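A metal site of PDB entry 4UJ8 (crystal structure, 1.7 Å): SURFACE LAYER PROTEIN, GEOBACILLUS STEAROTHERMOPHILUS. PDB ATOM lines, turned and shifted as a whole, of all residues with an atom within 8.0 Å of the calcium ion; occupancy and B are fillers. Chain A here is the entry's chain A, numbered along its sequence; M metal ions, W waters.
The side-chain hydroxyl (OG) of Ser 162 lies close to the backbone NH (N) of Ala 164, at 3.2 Å.
Of the 15 residues printed, 5 come within 4 Å of the calcium ion.
The calcium ion is bound by O of Ser 162, at 2.4 Å. OD1 of Asp 161 binds the calcium ion (2.4 Å). The calcium ion is bound by O of Thr 168 (2.4 Å). The calcium ion is bound by O of Thr 165 (2.4 Å). The calcium ion is bound by water W1. OG1 of Thr 165 binds the calcium ion, 2.5 Å away. OE1 of Glu 170 binds the calcium ion, at 2.9 Å. The calcium ion has seven donor atoms within binding distance.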
ATOM      1  N   VAL A 160      -7.379  21.088  26.902  1.00  0.00           N
ATOM      2  CA  VAL A 160      -7.368  19.883  27.725  1.00  0.00           C
ATOM      3  C   VAL A 160      -7.084  18.618  26.913  1.00  0.00           C
ATOM      4  O   VAL A 160      -7.113  18.631  25.678  1.00  0.00           O
ATOM      5  CB  VAL A 160      -8.712  19.712  28.473  1.00  0.00           C
ATOM      6  CG1 VAL A 160      -8.970  20.878  29.408  1.00  0.00           C
ATOM      7  CG2 VAL A 160      -9.844  19.546  27.486  1.00  0.00           C
ATOM      8  N   ASP A 161      -6.797  17.527  27.613  1.00  0.00           N
ATOM      9  CA  ASP A 161      -6.551  16.248  26.969  1.00  0.00           C
ATOM     10  C   ASP A 161      -7.877  15.706  26.435  1.00  0.00           C
ATOM     11  O   ASP A 161      -8.902  15.746  27.119  1.00  0.00           O
ATOM     12  CB  ASP A 161      -5.919  15.255  27.957  1.00  0.00           C
ATOM     13  CG  ASP A 161      -5.496  13.949  27.291  1.00  0.00           C
ATOM     14  OD1 ASP A 161      -5.245  13.940  26.073  1.00  0.00           O
ATOM     15  OD2 ASP A 161      -5.403  12.925  28.001  1.00  0.00           O
ATOM     16  N   SER A 162      -7.865  15.231  25.202  1.00  0.00           N
ATOM     17  CA  SER A 162      -9.036  14.559  24.663  1.00  0.00           C
ATOM     18  C   SER A 162      -8.926  13.076  24.944  1.00  0.00           C
ATOM     19  O   SER A 162      -7.901  12.467  24.637  1.00  0.00           O
ATOM     20  CB  SER A 162      -9.170  14.805  23.158  1.00  0.00           C
ATOM     21  OG  SER A 162     -10.101  13.895  22.580  1.00  0.00           O
ATOM     22  N   ALA A 163      -9.965  12.484  25.522  1.00  0.00           N
ATOM     23  CA  ALA A 163      -9.935  11.061  25.834  1.00  0.00           C
ATOM     24  C   ALA A 163     -10.057  10.213  24.577  1.00  0.00           C
ATOM     25  O   ALA A 163      -9.829   9.001  24.599  1.00  0.00           O
ATOM     26  CB  ALA A 163     -11.025  10.711  26.827  1.00  0.00           C
ATOM     27  N   ALA A 164     -10.410  10.851  23.459  1.00  0.00           N
ATOM     28  CA  ALA A 164     -10.578  10.138  22.195  1.00  0.00           C
ATOM     29  C   ALA A 164      -9.235   9.667  21.632  1.00  0.00           C
ATOM     30  O   ALA A 164      -9.199   8.806  20.762  1.00  0.00           O
ATOM     31  CB  ALA A 164     -11.297  11.015  21.188  1.00  0.00           C
ATOM     32  N   THR A 165      -8.152  10.252  22.131  1.00  0.00           N
ATOM     33  CA  THR A 165      -6.802   9.881  21.689  1.00  0.00           C
ATOM     34  C   THR A 165      -5.976   9.349  22.859  1.00  0.00           C
ATOM     35  O   THR A 165      -5.442  10.121  23.661  1.00  0.00           O
ATOM     36  CB  THR A 165      -6.082  11.071  21.043  1.00  0.00           C
ATOM     37  OG1 THR A 165      -6.219  12.221  21.893  1.00  0.00           O
ATOM     38  CG2 THR A 165      -6.671  11.393  19.678  1.00  0.00           C
ATOM     39  N   PRO A 166      -5.858   8.016  22.963  1.00  0.00           N
ATOM     40  CA  PRO A 166      -5.217   7.425  24.147  1.00  0.00           C
ATOM     41  C   PRO A 166      -3.693   7.644  24.234  1.00  0.00           C
ATOM     42  O   PRO A 166      -3.155   7.591  25.330  1.00  0.00           O
ATOM     43  CB  PRO A 166      -5.532   5.938  23.994  1.00  0.00           C
ATOM     44  CG  PRO A 166      -5.679   5.738  22.528  1.00  0.00           C
ATOM     45  CD  PRO A 166      -6.327   6.996  22.016  1.00  0.00           C
ATOM     46  N   ASN A 167      -3.024   7.904  23.111  1.00  0.00           N
ATOM     47  CA  ASN A 167      -1.556   7.909  23.109  1.00  0.00           C
ATOM     48  C   ASN A 167      -0.907   9.294  23.007  1.00  0.00           C
ATOM     49  O   ASN A 167       0.318   9.401  22.928  1.00  0.00           O
ATOM     50  CB  ASN A 167      -1.041   7.037  21.968  1.00  0.00           C
ATOM     51  CG  ASN A 167      -1.280   5.556  22.220  1.00  0.00           C
ATOM     52  OD1 ASN A 167      -1.299   5.108  23.362  1.00  0.00           O
ATOM     53  ND2 ASN A 167      -1.462   4.807  21.149  1.00  0.00           N
ATOM     54  N   THR A 168      -1.718  10.336  22.989  1.00  0.00           N
ATOM     55  CA  THR A 168      -1.200  11.704  22.945  1.00  0.00           C
ATOM     56  C   THR A 168      -2.016  12.588  23.879  1.00  0.00           C
ATOM     57  O   THR A 168      -3.230  12.572  23.837  1.00  0.00           O
ATOM     58  CB  THR A 168      -1.210  12.296  21.509  1.00  0.00           C
ATOM     59  OG1 THR A 168      -2.555  12.583  21.109  1.00  0.00           O
ATOM     60  CG2 THR A 168      -0.563  11.337  20.508  1.00  0.00           C
ATOM     61  N   ASN A 169      -1.325  13.332  24.740  1.00  0.00           N
ATOM     62  CA  ASN A 169      -1.980  14.256  25.634  1.00  0.00           C
ATOM     63  C   ASN A 169      -1.947  15.673  25.050  1.00  0.00           C
ATOM     64  O   ASN A 169      -0.900  16.324  25.056  1.00  0.00           O
ATOM     65  CB  ASN A 169      -1.307  14.223  27.007  1.00  0.00           C
ATOM     66  CG  ASN A 169      -2.039  15.048  28.044  1.00  0.00           C
ATOM     67  OD1 ASN A 169      -2.388  16.207  27.787  1.00  0.00           O
ATOM     68  ND2 ASN A 169      -2.289  14.458  29.212  1.00  0.00           N
ATOM     69  N   GLU A 170      -3.088  16.131  24.522  1.00  0.00           N
ATOM     70  CA  GLU A 170      -3.173  17.437  23.865  1.00  0.00           C
ATOM     71  C   GLU A 170      -2.832  18.598  24.815  1.00  0.00           C
ATOM     72  O   GLU A 170      -2.350  19.644  24.388  1.00  0.00           O
ATOM     73  CB  GLU A 170      -4.561  17.654  23.277  1.00  0.00           C
ATOM     74  CG  GLU A 170      -4.787  16.965  21.942  1.00  0.00           C
ATOM     75  CD  GLU A 170      -5.331  15.550  22.059  1.00  0.00           C
ATOM     76  OE1 GLU A 170      -5.631  15.107  23.199  1.00  0.00           O
ATOM     77  OE2 GLU A 170      -5.467  14.880  21.012  1.00  0.00           O
ATOM     78  N   LYS A 171      -3.105  18.418  26.099  1.00  0.00           N
ATOM     79  CA  LYS A 171      -2.768  19.450  27.083  1.00  0.00           C
ATOM     80  C   LYS A 171      -1.247  19.559  27.283  1.00  0.00           C
ATOM     81  O   LYS A 171      -0.703  20.673  27.318  1.00  0.00           O
ATOM     82  CB  LYS A 171      -3.461  19.157  28.422  1.00  0.00           C
ATOM     83  CG  LYS A 171      -3.261  20.234  29.473  1.00  0.00           C
ATOM     84  CD  LYS A 171      -4.000  19.891  30.767  1.00  0.00           C
ATOM     85  CE  LYS A 171      -3.561  20.820  31.916  1.00  0.00           C
ATOM     86  NZ  LYS A 171      -4.253  20.497  33.183  1.00  0.00           N
ATOM     87  N   ASP A 201       5.290  12.746  25.461  1.00  0.00           N
ATOM     88  CA  ASP A 201       3.888  12.550  25.182  1.00  0.00           C
ATOM     89  C   ASP A 201       3.648  11.079  24.885  1.00  0.00           C
ATOM     90  O   ASP A 201       4.297  10.494  24.032  1.00  0.00           O
ATOM     91  CB  ASP A 201       3.469  13.433  23.997  1.00  0.00           C
ATOM     92  CG  ASP A 201       1.980  13.424  23.760  1.00  0.00           C
ATOM     93  OD1 ASP A 201       1.219  13.117  24.707  1.00  0.00           O
ATOM     94  OD2 ASP A 201       1.577  13.736  22.629  1.00  0.00           O
ATOM     95  N   ASP A 202       2.696  10.493  25.610  1.00  0.00           N
ATOM     96  CA  ASP A 202       2.442   9.063  25.543  1.00  0.00           C
ATOM     97  C   ASP A 202       1.146   8.811  26.319  1.00  0.00           C
ATOM     98  O   ASP A 202       0.608   9.740  26.915  1.00  0.00           O
ATOM     99  CB  ASP A 202       3.622   8.272  26.119  1.00  0.00           C
ATOM    100  CG  ASP A 202       3.437   6.773  26.022  1.00  0.00           C
ATOM    101  OD1 ASP A 202       3.420   6.246  24.885  1.00  0.00           O
ATOM    102  OD2 ASP A 202       3.289   6.111  27.085  1.00  0.00           O
ATOM    103  N   ALA A 203       0.649   7.573  26.312  1.00  0.00           N
ATOM    104  CA  ALA A 203      -0.499   7.217  27.148  1.00  0.00           C
ATOM    105  C   ALA A 203      -0.215   7.540  28.614  1.00  0.00           C
ATOM    106  O   ALA A 203      -1.093   8.002  29.336  1.00  0.00           O
ATOM    107  CB  ALA A 203      -0.838   5.734  26.998  1.00  0.00           C
HETATM  108 CA    CA M   1      -5.568  12.426  24.275  1.00  0.00          CA
HETATM  109  O   HOH W   1      -5.183  11.123  26.242  1.00  0.00           O
